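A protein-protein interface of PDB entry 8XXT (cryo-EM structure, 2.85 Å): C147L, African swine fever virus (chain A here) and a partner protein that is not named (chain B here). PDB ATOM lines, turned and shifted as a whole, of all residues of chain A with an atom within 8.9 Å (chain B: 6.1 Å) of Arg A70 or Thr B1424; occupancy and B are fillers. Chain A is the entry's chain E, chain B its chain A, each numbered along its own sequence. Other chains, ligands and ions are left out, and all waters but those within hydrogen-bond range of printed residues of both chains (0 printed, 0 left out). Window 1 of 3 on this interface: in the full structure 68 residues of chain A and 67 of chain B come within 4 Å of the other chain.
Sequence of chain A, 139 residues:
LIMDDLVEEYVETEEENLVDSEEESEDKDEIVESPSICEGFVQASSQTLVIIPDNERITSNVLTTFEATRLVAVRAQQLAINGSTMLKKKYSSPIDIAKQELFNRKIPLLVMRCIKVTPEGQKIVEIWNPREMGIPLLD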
ATOM      1  N   LEU A  63     -26.657  20.632 -29.187  1.00  0.00           N
ATOM      2  CA  LEU A  63     -25.618  21.642 -29.068  1.00  0.00           C
ATOM      3  C   LEU A  63     -26.035  22.918 -29.783  1.00  0.00           C
ATOM      4  O   LEU A  63     -26.566  22.883 -30.894  1.00  0.00           O
ATOM      5  CB  LEU A  63     -24.307  21.129 -29.658  1.00  0.00           C
ATOM      6  CG  LEU A  63     -23.548  20.052 -28.894  1.00  0.00           C
ATOM      7  CD1 LEU A  63     -22.639  19.306 -29.838  1.00  0.00           C
ATOM      8  CD2 LEU A  63     -22.750  20.675 -27.772  1.00  0.00           C
ATOM      9  N   THR A  64     -25.800  24.053 -29.135  1.00  0.00           N
ATOM     10  CA  THR A  64     -25.945  25.321 -29.824  1.00  0.00           C
ATOM     11  C   THR A  64     -24.813  25.486 -30.831  1.00  0.00           C
ATOM     12  O   THR A  64     -23.761  24.853 -30.726  1.00  0.00           O
ATOM     13  CB  THR A  64     -25.938  26.481 -28.832  1.00  0.00           C
ATOM     14  OG1 THR A  64     -24.652  26.571 -28.213  1.00  0.00           O
ATOM     15  CG2 THR A  64     -26.982  26.258 -27.758  1.00  0.00           C
ATOM     16  N   THR A  65     -25.046  26.335 -31.833  1.00  0.00           N
ATOM     17  CA  THR A  65     -23.989  26.614 -32.798  1.00  0.00           C
ATOM     18  C   THR A  65     -22.750  27.159 -32.107  1.00  0.00           C
ATOM     19  O   THR A  65     -21.624  26.858 -32.517  1.00  0.00           O
ATOM     20  CB  THR A  65     -24.479  27.597 -33.855  1.00  0.00           C
ATOM     21  OG1 THR A  65     -25.142  28.693 -33.217  1.00  0.00           O
ATOM     22  CG2 THR A  65     -25.442  26.915 -34.799  1.00  0.00           C
ATOM     23  N   PHE A  66     -22.941  27.946 -31.049  1.00  0.00           N
ATOM     24  CA  PHE A  66     -21.815  28.429 -30.263  1.00  0.00           C
ATOM     25  C   PHE A  66     -21.040  27.275 -29.641  1.00  0.00           C
ATOM     26  O   PHE A  66     -19.812  27.209 -29.749  1.00  0.00           O
ATOM     27  CB  PHE A  66     -22.318  29.375 -29.178  1.00  0.00           C
ATOM     28  CG  PHE A  66     -22.881  30.657 -29.701  1.00  0.00           C
ATOM     29  CD1 PHE A  66     -22.272  31.319 -30.745  1.00  0.00           C
ATOM     30  CD2 PHE A  66     -24.019  31.204 -29.142  1.00  0.00           C
ATOM     31  CE1 PHE A  66     -22.790  32.502 -31.225  1.00  0.00           C
ATOM     32  CE2 PHE A  66     -24.537  32.384 -29.617  1.00  0.00           C
ATOM     33  CZ  PHE A  66     -23.923  33.033 -30.660  1.00  0.00           C
ATOM     34  N   GLU A  67     -21.746  26.351 -28.982  1.00  0.00           N
ATOM     35  CA  GLU A  67     -21.073  25.251 -28.300  1.00  0.00           C
ATOM     36  C   GLU A  67     -20.424  24.293 -29.288  1.00  0.00           C
ATOM     37  O   GLU A  67     -19.312  23.813 -29.051  1.00  0.00           O
ATOM     38  CB  GLU A  67     -22.056  24.505 -27.403  1.00  0.00           C
ATOM     39  CG  GLU A  67     -22.459  25.277 -26.166  1.00  0.00           C
ATOM     40  CD  GLU A  67     -23.587  24.620 -25.405  1.00  0.00           C
ATOM     41  OE1 GLU A  67     -24.434  23.963 -26.040  1.00  0.00           O
ATOM     42  OE2 GLU A  67     -23.633  24.765 -24.167  1.00  0.00           O
ATOM     43  N   ALA A  68     -21.104  23.991 -30.393  1.00  0.00           N
ATOM     44  CA  ALA A  68     -20.504  23.131 -31.406  1.00  0.00           C
ATOM     45  C   ALA A  68     -19.265  23.777 -32.010  1.00  0.00           C
ATOM     46  O   ALA A  68     -18.244  23.110 -32.214  1.00  0.00           O
ATOM     47  CB  ALA A  68     -21.528  22.808 -32.490  1.00  0.00           C
ATOM     48  N   THR A  69     -19.334  25.078 -32.296  1.00  0.00           N
ATOM     49  CA  THR A  69     -18.173  25.782 -32.824  1.00  0.00           C
ATOM     50  C   THR A  69     -17.024  25.771 -31.827  1.00  0.00           C
ATOM     51  O   THR A  69     -15.866  25.585 -32.208  1.00  0.00           O
ATOM     52  CB  THR A  69     -18.552  27.216 -33.185  1.00  0.00           C
ATOM     53  OG1 THR A  69     -19.647  27.200 -34.105  1.00  0.00           O
ATOM     54  CG2 THR A  69     -17.380  27.932 -33.819  1.00  0.00           C
ATOM     55  N   ARG A  70     -17.327  25.975 -30.545  1.00  0.00           N
ATOM     56  CA  ARG A  70     -16.287  25.947 -29.525  1.00  0.00           C
ATOM     57  C   ARG A  70     -15.651  24.568 -29.422  1.00  0.00           C
ATOM     58  O   ARG A  70     -14.428  24.450 -29.297  1.00  0.00           O
ATOM     59  CB  ARG A  70     -16.866  26.369 -28.180  1.00  0.00           C
ATOM     60  CG  ARG A  70     -15.894  26.254 -27.036  1.00  0.00           C
ATOM     61  CD  ARG A  70     -14.820  27.310 -27.112  1.00  0.00           C
ATOM     62  NE  ARG A  70     -13.983  27.299 -25.920  1.00  0.00           N
ATOM     63  CZ  ARG A  70     -12.782  27.852 -25.846  1.00  0.00           C
ATOM     64  NH1 ARG A  70     -12.253  28.494 -26.872  1.00  0.00           N
ATOM     65  NH2 ARG A  70     -12.096  27.758 -24.713  1.00  0.00           N
ATOM     66  N   LEU A  71     -16.467  23.513 -29.471  1.00  0.00           N
ATOM     67  CA  LEU A  71     -15.929  22.159 -29.436  1.00  0.00           C
ATOM     68  C   LEU A  71     -15.000  21.913 -30.614  1.00  0.00           C
ATOM     69  O   LEU A  71     -13.894  21.388 -30.450  1.00  0.00           O
ATOM     70  CB  LEU A  71     -17.064  21.139 -29.444  1.00  0.00           C
ATOM     71  CG  LEU A  71     -17.883  20.969 -28.174  1.00  0.00           C
ATOM     72  CD1 LEU A  71     -19.159  20.235 -28.496  1.00  0.00           C
ATOM     73  CD2 LEU A  71     -17.087  20.215 -27.144  1.00  0.00           C
ATOM     74  N   VAL A  72     -15.437  22.297 -31.815  1.00  0.00           N
ATOM     75  CA  VAL A  72     -14.618  22.064 -33.000  1.00  0.00           C
ATOM     76  C   VAL A  72     -13.327  22.865 -32.922  1.00  0.00           C
ATOM     77  O   VAL A  72     -12.254  22.364 -33.266  1.00  0.00           O
ATOM     78  CB  VAL A  72     -15.408  22.385 -34.278  1.00  0.00           C
ATOM     79  CG1 VAL A  72     -14.538  22.166 -35.491  1.00  0.00           C
ATOM     80  CG2 VAL A  72     -16.623  21.509 -34.365  1.00  0.00           C
ATOM     81  N   ALA A  73     -13.404  24.116 -32.466  1.00  0.00           N
ATOM     82  CA  ALA A  73     -12.209  24.950 -32.380  1.00  0.00           C
ATOM     83  C   ALA A  73     -11.217  24.393 -31.370  1.00  0.00           C
ATOM     84  O   ALA A  73     -10.011  24.326 -31.636  1.00  0.00           O
ATOM     85  CB  ALA A  73     -12.599  26.382 -32.019  1.00  0.00           C
ATOM     86  N   VAL A  74     -11.710  23.982 -30.201  1.00  0.00           N
ATOM     87  CA  VAL A  74     -10.835  23.429 -29.172  1.00  0.00           C
ATOM     88  C   VAL A  74     -10.184  22.145 -29.665  1.00  0.00           C
ATOM     89  O   VAL A  74      -8.974  21.937 -29.507  1.00  0.00           O
ATOM     90  CB  VAL A  74     -11.622  23.198 -27.871  1.00  0.00           C
ATOM     91  CG1 VAL A  74     -10.852  22.290 -26.943  1.00  0.00           C
ATOM     92  CG2 VAL A  74     -11.922  24.517 -27.199  1.00  0.00           C
ATOM     93  N   ARG A  75     -10.977  21.267 -30.282  1.00  0.00           N
ATOM     94  CA  ARG A  75     -10.428  20.015 -30.784  1.00  0.00           C
ATOM     95  C   ARG A  75      -9.420  20.261 -31.894  1.00  0.00           C
ATOM     96  O   ARG A  75      -8.398  19.575 -31.974  1.00  0.00           O
ATOM     97  CB  ARG A  75     -11.551  19.108 -31.272  1.00  0.00           C
ATOM     98  CG  ARG A  75     -11.061  17.804 -31.849  1.00  0.00           C
ATOM     99  CD  ARG A  75     -10.897  16.766 -30.764  1.00  0.00           C
ATOM    100  NE  ARG A  75      -9.794  15.855 -31.040  1.00  0.00           N
ATOM    101  CZ  ARG A  75      -8.714  15.741 -30.281  1.00  0.00           C
ATOM    102  NH1 ARG A  75      -8.569  16.450 -29.175  1.00  0.00           N
ATOM    103  NH2 ARG A  75      -7.757  14.891 -30.640  1.00  0.00           N
ATOM    104  N   ALA A  76      -9.687  21.232 -32.767  1.00  0.00           N
ATOM    105  CA  ALA A  76      -8.759  21.534 -33.848  1.00  0.00           C
ATOM    106  C   ALA A  76      -7.449  22.092 -33.312  1.00  0.00           C
ATOM    107  O   ALA A  76      -6.373  21.750 -33.810  1.00  0.00           O
ATOM    108  CB  ALA A  76      -9.404  22.505 -34.830  1.00  0.00           C
ATOM    109  N   GLN A  77      -7.511  22.944 -32.289  1.00  0.00           N
ATOM    110  CA  GLN A  77      -6.275  23.437 -31.690  1.00  0.00           C
ATOM    111  C   GLN A  77      -5.495  22.308 -31.027  1.00  0.00           C
ATOM    112  O   GLN A  77      -4.267  22.227 -31.157  1.00  0.00           O
ATOM    113  CB  GLN A  77      -6.576  24.540 -30.681  1.00  0.00           C
ATOM    114  CG  GLN A  77      -5.332  25.191 -30.127  1.00  0.00           C
ATOM    115  CD  GLN A  77      -4.454  25.771 -31.210  1.00  0.00           C
ATOM    116  OE1 GLN A  77      -4.875  26.644 -31.966  1.00  0.00           O
ATOM    117  NE2 GLN A  77      -3.225  25.283 -31.299  1.00  0.00           N
ATOM    118  N   GLN A  78      -6.193  21.418 -30.320  1.00  0.00           N
ATOM    119  CA  GLN A  78      -5.501  20.310 -29.675  1.00  0.00           C
ATOM    120  C   GLN A  78      -4.937  19.331 -30.694  1.00  0.00           C
ATOM    121  O   GLN A  78      -3.923  18.681 -30.429  1.00  0.00           O
ATOM    122  CB  GLN A  78      -6.434  19.601 -28.704  1.00  0.00           C
ATOM    123  CG  GLN A  78      -6.776  20.444 -27.499  1.00  0.00           C
ATOM    124  CD  GLN A  78      -7.805  19.795 -26.618  1.00  0.00           C
ATOM    125  OE1 GLN A  78      -8.276  18.697 -26.901  1.00  0.00           O
ATOM    126  NE2 GLN A  78      -8.159  20.467 -25.536  1.00  0.00           N
ATOM    127  N   ALA A  98     -11.355  17.811 -36.758  1.00  0.00           N
ATOM    128  CA  ALA A  98     -12.215  18.137 -35.627  1.00  0.00           C
ATOM    129  C   ALA A  98     -13.680  18.179 -36.038  1.00  0.00           C
ATOM    130  O   ALA A  98     -14.555  17.709 -35.300  1.00  0.00           O
ATOM    131  CB  ALA A  98     -11.793  19.469 -35.016  1.00  0.00           C
ATOM    132  N   LEU A 102     -16.623  15.733 -34.611  1.00  0.00           N
ATOM    133  CA  LEU A 102     -17.899  16.171 -34.052  1.00  0.00           C
ATOM    134  C   LEU A 102     -19.074  15.513 -34.767  1.00  0.00           C
ATOM    135  O   LEU A 102     -20.026  15.064 -34.119  1.00  0.00           O
ATOM    136  CB  LEU A 102     -18.021  17.691 -34.127  1.00  0.00           C
ATOM    137  CG  LEU A 102     -19.329  18.234 -33.550  1.00  0.00           C
ATOM    138  CD1 LEU A 102     -19.310  18.202 -32.032  1.00  0.00           C
ATOM    139  CD2 LEU A 102     -19.609  19.630 -34.059  1.00  0.00           C
ATOM    140  N   ILE A 107     -15.748  12.861 -30.480  1.00  0.00           N
ATOM    141  CA  ILE A 107     -14.932  13.979 -30.013  1.00  0.00           C
ATOM    142  C   ILE A 107     -14.618  13.759 -28.535  1.00  0.00           C
ATOM    143  O   ILE A 107     -15.513  13.417 -27.750  1.00  0.00           O
ATOM    144  CB  ILE A 107     -15.624  15.326 -30.296  1.00  0.00           C
ATOM    145  CG1 ILE A 107     -14.592  16.448 -30.409  1.00  0.00           C
ATOM    146  CG2 ILE A 107     -16.688  15.660 -29.260  1.00  0.00           C
ATOM    147  CD1 ILE A 107     -14.978  17.524 -31.390  1.00  0.00           C
ATOM    148  N   LEU A 109     -14.261  15.505 -25.956  1.00  0.00           N
ATOM    149  CA  LEU A 109     -14.497  16.709 -25.179  1.00  0.00           C
ATOM    150  C   LEU A 109     -15.882  16.635 -24.563  1.00  0.00           C
ATOM    151  O   LEU A 109     -16.785  16.007 -25.115  1.00  0.00           O
ATOM    152  CB  LEU A 109     -14.384  17.971 -26.043  1.00  0.00           C
ATOM    153  CG  LEU A 109     -13.077  18.200 -26.800  1.00  0.00           C
ATOM    154  CD1 LEU A 109     -13.196  19.401 -27.703  1.00  0.00           C
ATOM    155  CD2 LEU A 109     -11.934  18.383 -25.836  1.00  0.00           C
ATOM    156  N   LEU A 110     -16.039  17.276 -23.413  1.00  0.00           N
ATOM    157  CA  LEU A 110     -17.323  17.357 -22.741  1.00  0.00           C
ATOM    158  C   LEU A 110     -17.723  18.814 -22.598  1.00  0.00           C
ATOM    159  O   LEU A 110     -16.878  19.690 -22.411  1.00  0.00           O
ATOM    160  CB  LEU A 110     -17.284  16.698 -21.364  1.00  0.00           C
ATOM    161  CG  LEU A 110     -17.193  15.179 -21.310  1.00  0.00           C
ATOM    162  CD1 LEU A 110     -17.166  14.727 -19.873  1.00  0.00           C
ATOM    163  CD2 LEU A 110     -18.355  14.552 -22.041  1.00  0.00           C
ATOM    164  N   VAL A 111     -19.021  19.066 -22.688  1.00  0.00           N
ATOM    165  CA  VAL A 111     -19.570  20.408 -22.561  1.00  0.00           C
ATOM    166  C   VAL A 111     -20.118  20.546 -21.150  1.00  0.00           C
ATOM    167  O   VAL A 111     -21.093  19.883 -20.785  1.00  0.00           O
ATOM    168  CB  VAL A 111     -20.657  20.680 -23.607  1.00  0.00           C
ATOM    169  CG1 VAL A 111     -21.394  21.958 -23.270  1.00  0.00           C
ATOM    170  CG2 VAL A 111     -20.043  20.770 -24.984  1.00  0.00           C
ATOM    171  N   PRO A 130     -21.125  15.574 -25.982  1.00  0.00           N
ATOM    172  CA  PRO A 130     -21.396  15.941 -27.380  1.00  0.00           C
ATOM    173  C   PRO A 130     -21.647  14.756 -28.285  1.00  0.00           C
ATOM    174  O   PRO A 130     -22.297  14.916 -29.323  1.00  0.00           O
ATOM    175  CB  PRO A 130     -20.127  16.695 -27.798  1.00  0.00           C
ATOM    176  CG  PRO A 130     -19.494  17.114 -26.531  1.00  0.00           C
ATOM    177  CD  PRO A 130     -19.817  16.058 -25.530  1.00  0.00           C
ATOM    178  N   PRO A 136     -25.985  20.944 -34.426  1.00  0.00           N
ATOM    179  CA  PRO A 136     -26.657  21.950 -35.255  1.00  0.00           C
ATOM    180  C   PRO A 136     -26.253  21.864 -36.717  1.00  0.00           C
ATOM    181  O   PRO A 136     -25.535  20.942 -37.119  1.00  0.00           O
ATOM    182  CB  PRO A 136     -26.214  23.274 -34.624  1.00  0.00           C
ATOM    183  CG  PRO A 136     -24.948  22.954 -33.929  1.00  0.00           C
ATOM    184  CD  PRO A 136     -25.096  21.558 -33.429  1.00  0.00           C
ATOM    185  N   LEU A 138     -24.343  23.998 -38.883  1.00  0.00           N
ATOM    186  CA  LEU A 138     -22.910  24.226 -39.051  1.00  0.00           C
ATOM    187  C   LEU A 138     -22.487  24.196 -40.516  1.00  0.00           C
ATOM    188  O   LEU A 138     -21.298  24.313 -40.824  1.00  0.00           O
ATOM    189  CB  LEU A 138     -22.103  23.197 -38.254  1.00  0.00           C
ATOM    190  CG  LEU A 138     -22.245  23.221 -36.733  1.00  0.00           C
ATOM    191  CD1 LEU A 138     -21.152  22.388 -36.100  1.00  0.00           C
ATOM    192  CD2 LEU A 138     -22.207  24.643 -36.208  1.00  0.00           C
ATOM    193  N   MET B 472      -8.387  28.287 -33.862  1.00  0.00           N
ATOM    194  CA  MET B 472      -9.646  28.573 -33.183  1.00  0.00           C
ATOM    195  C   MET B 472     -10.434  29.653 -33.908  1.00  0.00           C
ATOM    196  O   MET B 472     -11.660  29.561 -34.029  1.00  0.00           O
ATOM    197  CB  MET B 472      -9.387  28.986 -31.737  1.00  0.00           C
ATOM    198  CG  MET B 472      -8.853  27.886 -30.845  1.00  0.00           C
ATOM    199  SD  MET B 472      -9.821  27.782 -29.331  1.00  0.00           S
ATOM    200  CE  MET B 472      -8.736  26.828 -28.289  1.00  0.00           C
ATOM    201  N   GLU B 476     -13.882  29.027 -36.072  1.00  0.00           N
ATOM    202  CA  GLU B 476     -14.982  29.923 -35.753  1.00  0.00           C
ATOM    203  C   GLU B 476     -15.476  30.684 -36.974  1.00  0.00           C
ATOM    204  O   GLU B 476     -16.686  30.816 -37.181  1.00  0.00           O
ATOM    205  CB  GLU B 476     -14.510  30.896 -34.691  1.00  0.00           C
ATOM    206  CG  GLU B 476     -15.234  32.178 -34.713  1.00  0.00           C
ATOM    207  CD  GLU B 476     -15.459  32.703 -33.352  1.00  0.00           C
ATOM    208  OE1 GLU B 476     -15.390  31.924 -32.382  1.00  0.00           O
ATOM    209  OE2 GLU B 476     -15.633  33.922 -33.258  1.00  0.00           O
ATOM    210  N   LEU B 480     -19.318  29.949 -37.754  1.00  0.00           N
ATOM    211  CA  LEU B 480     -20.210  30.845 -37.029  1.00  0.00           C
ATOM    212  C   LEU B 480     -20.435  32.182 -37.710  1.00  0.00           C
ATOM    213  O   LEU B 480     -21.568  32.658 -37.756  1.00  0.00           O
ATOM    214  CB  LEU B 480     -19.662  31.089 -35.622  1.00  0.00           C
ATOM    215  CG  LEU B 480     -20.602  31.775 -34.639  1.00  0.00           C
ATOM    216  CD1 LEU B 480     -21.659  30.799 -34.171  1.00  0.00           C
ATOM    217  CD2 LEU B 480     -19.808  32.312 -33.472  1.00  0.00           C
ATOM    218  N   TYR B1037     -27.830  29.627 -26.269  1.00  0.00           N
ATOM    219  CA  TYR B1037     -27.300  30.050 -24.984  1.00  0.00           C
ATOM    220  C   TYR B1037     -26.095  30.956 -25.188  1.00  0.00           C
ATOM    221  O   TYR B1037     -25.239  30.699 -26.038  1.00  0.00           O
ATOM    222  CB  TYR B1037     -26.897  28.835 -24.156  1.00  0.00           C
ATOM    223  CG  TYR B1037     -27.978  27.800 -24.008  1.00  0.00           C
ATOM    224  CD1 TYR B1037     -29.290  28.172 -23.791  1.00  0.00           C
ATOM    225  CD2 TYR B1037     -27.684  26.449 -24.075  1.00  0.00           C
ATOM    226  CE1 TYR B1037     -30.277  27.231 -23.642  1.00  0.00           C
ATOM    227  CE2 TYR B1037     -28.668  25.501 -23.930  1.00  0.00           C
ATOM    228  CZ  TYR B1037     -29.961  25.900 -23.711  1.00  0.00           C
ATOM    229  OH  TYR B1037     -30.955  24.968 -23.563  1.00  0.00           O
ATOM    230  N   GLY B1038     -26.027  32.024 -24.402  1.00  0.00           N
ATOM    231  CA  GLY B1038     -24.880  32.900 -24.446  1.00  0.00           C
ATOM    232  C   GLY B1038     -24.879  33.915 -25.560  1.00  0.00           C
ATOM    233  O   GLY B1038     -23.872  34.603 -25.744  1.00  0.00           O
ATOM    234  N   ILE B1422     -19.541  35.050 -23.452  1.00  0.00           N
ATOM    235  CA  ILE B1422     -20.762  34.964 -24.242  1.00  0.00           C
ATOM    236  C   ILE B1422     -20.548  33.888 -25.293  1.00  0.00           C
ATOM    237  O   ILE B1422     -19.536  33.179 -25.265  1.00  0.00           O
ATOM    238  CB  ILE B1422     -21.161  36.301 -24.885  1.00  0.00           C
ATOM    239  CG1 ILE B1422     -20.057  36.783 -25.799  1.00  0.00           C
ATOM    240  CG2 ILE B1422     -21.473  37.341 -23.827  1.00  0.00           C
ATOM    241  CD1 ILE B1422     -20.448  37.925 -26.640  1.00  0.00           C
ATOM    242  N   GLY B1423     -21.472  33.792 -26.244  1.00  0.00           N
ATOM    243  CA  GLY B1423     -21.804  32.551 -26.917  1.00  0.00           C
ATOM    244  C   GLY B1423     -20.724  31.519 -27.158  1.00  0.00           C
ATOM    245  O   GLY B1423     -20.839  30.403 -26.642  1.00  0.00           O
ATOM    246  N   THR B1424     -19.670  31.850 -27.904  1.00  0.00           N
ATOM    247  CA  THR B1424     -18.668  30.830 -28.193  1.00  0.00           C
ATOM    248  C   THR B1424     -18.008  30.327 -26.920  1.00  0.00           C
ATOM    249  O   THR B1424     -17.783  29.123 -26.772  1.00  0.00           O
ATOM    250  CB  THR B1424     -17.624  31.364 -29.167  1.00  0.00           C
ATOM    251  OG1 THR B1424     -18.119  31.243 -30.505  1.00  0.00           O
ATOM    252  CG2 THR B1424     -16.341  30.583 -29.060  1.00  0.00           C
ATOM    253  N   MET B1425     -17.732  31.220 -25.976  1.00  0.00           N
ATOM    254  CA  MET B1425     -17.108  30.845 -24.718  1.00  0.00           C
ATOM    255  C   MET B1425     -18.078  30.911 -23.548  1.00  0.00           C
ATOM    256  O   MET B1425     -17.652  31.024 -22.398  1.00  0.00           O
ATOM    257  CB  MET B1425     -15.895  31.729 -24.470  1.00  0.00           C
ATOM    258  CG  MET B1425     -15.039  31.866 -25.703  1.00  0.00           C
ATOM    259  SD  MET B1425     -13.347  32.183 -25.259  1.00  0.00           S
ATOM    260  CE  MET B1425     -13.620  33.653 -24.298  1.00  0.00           C
ATOM    261  N   TYR B1426     -19.379  30.848 -23.824  1.00  0.00           N
ATOM    262  CA  TYR B1426     -20.358  30.802 -22.747  1.00  0.00           C
ATOM    263  C   TYR B1426     -20.282  29.487 -21.988  1.00  0.00           C
ATOM    264  O   TYR B1426     -20.416  29.464 -20.760  1.00  0.00           O
ATOM    265  CB  TYR B1426     -21.761  31.012 -23.305  1.00  0.00           C
ATOM    266  CG  TYR B1426     -22.783  31.358 -22.254  1.00  0.00           C
ATOM    267  CD1 TYR B1426     -22.731  32.567 -21.584  1.00  0.00           C
ATOM    268  CD2 TYR B1426     -23.801  30.478 -21.935  1.00  0.00           C
ATOM    269  CE1 TYR B1426     -23.662  32.889 -20.625  1.00  0.00           C
ATOM    270  CE2 TYR B1426     -24.736  30.793 -20.977  1.00  0.00           C
ATOM    271  CZ  TYR B1426     -24.662  31.998 -20.325  1.00  0.00           C
ATOM    272  OH  TYR B1426     -25.589  32.318 -19.367  1.00  0.00           O
ATOM    273  N   SER B1427     -20.070  28.385 -22.698  1.00  0.00           N
ATOM    274  CA  SER B1427     -20.049  27.060 -22.099  1.00  0.00           C
ATOM    275  C   SER B1427     -18.618  26.567 -21.956  1.00  0.00           C
ATOM    276  O   SER B1427     -17.823  26.650 -22.896  1.00  0.00           O
ATOM    277  CB  SER B1427     -20.856  26.069 -22.935  1.00  0.00           C
ATOM    278  OG  SER B1427     -22.208  26.470 -23.036  1.00  0.00           O
ATOM    279  N   ILE B1429     -15.576  23.956 -21.756  1.00  0.00           N
ATOM    280  CA  ILE B1429     -15.189  22.703 -22.388  1.00  0.00           C
ATOM    281  C   ILE B1429     -14.184  22.018 -21.479  1.00  0.00           C
ATOM    282  O   ILE B1429     -13.209  22.640 -21.044  1.00  0.00           O
ATOM    283  CB  ILE B1429     -14.601  22.930 -23.789  1.00  0.00           C
ATOM    284  CG1 ILE B1429     -15.590  23.698 -24.657  1.00  0.00           C
ATOM    285  CG2 ILE B1429     -14.262  21.610 -24.438  1.00  0.00           C
ATOM    286  CD1 ILE B1429     -16.955  23.073 -24.729  1.00  0.00           C
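The side-chain hydroxyl (OG1) of Thr B1424 lies within hydrogen-bond range of the side-chain carboxylate (OE1) of Glu B476. O of Gly B1038 lies within hydrogen-bond range of N of Gly B1423 (2.6 Å). The side-chain hydroxyl (OG1) of Thr A64 is in hydrogen-bond range of the backbone NH (N) of Glu A67 (3.0 Å). O of Thr A65 lies within hydrogen-bond range of OG1 of Thr A69, 2.6 Å away.
Arg A70 touches just these residues of chain B: Met B472, Thr B1424 and Ile B1429. Thr B1424 touches just these residues of chain A: Phe A66 (3.8 Å) and Arg A70 (3.2 Å). Gly B1423 touches just one residue of chain A: Phe A66 (3.1 Å). Of the printed residues of chain B, Leu A71 touches Ile B1429. Of the printed residues of chain B, Leu A110 touches Ile B1429 (3.5 Å). Of the printed residues of chain A, Met B472 touches Arg A70 (3.5 Å), Ala A73 (3.8 Å) and Gln A77 (3.95 Å). Val A72 touches none of the printed residues of chain B. The nearest residue of chain B that does not touch Arg A70 is Met B1425 (4.2 Å).
The side-chain sulfur (SD) of Met B472 lies within hydrogen-bond range of the guanidinium group (NH1) of Arg A70, 3.5 Å away. The side-chain hydroxyl (OG) of Ser B1427 lies within hydrogen-bond range of the side-chain carboxylate (OE2) of Glu A67.
Of the 25 printed residues of chain A, 11 touch a printed residue of chain B. Printed residues of chain A that touch a printed residue of chain B: Thr A64, Phe A66, Glu A67, Thr A69, Arg A70, Leu A71, Ala A73, Gln A77, Leu A109, Leu A110 and Val A111. Of the 12 printed residues of chain B, 8 touch a printed residue of chain A. Hydrophobic or aromatic side chains of chain B that line the printed part of chain A: Met B472, Leu B480, Tyr B1037 and Ile B1429. Along chain B the printed residues that touch a printed residue of chain A span positions 472 to 1429.
CG2 of Thr A64 touches CD2 of Tyr B1037, at 3.8 Å. Phe A66 touches Tyr B1037. Gly B1423 touches Phe A66 (O to CB, 3.1 Å). Thr B1424 touches Phe A66. Thr A69 touches Glu B476 (CG2 to CA, 3.7 Å). CB of Arg A70 touches O of Thr B1424, 3.2 Å away. Leu A71 touches Ile B1429. Ala A73 touches Met B472. Gln A77 touches Met B472. Leu A109 touches Ile B1429 (CB to CG2, 3.98 Å).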
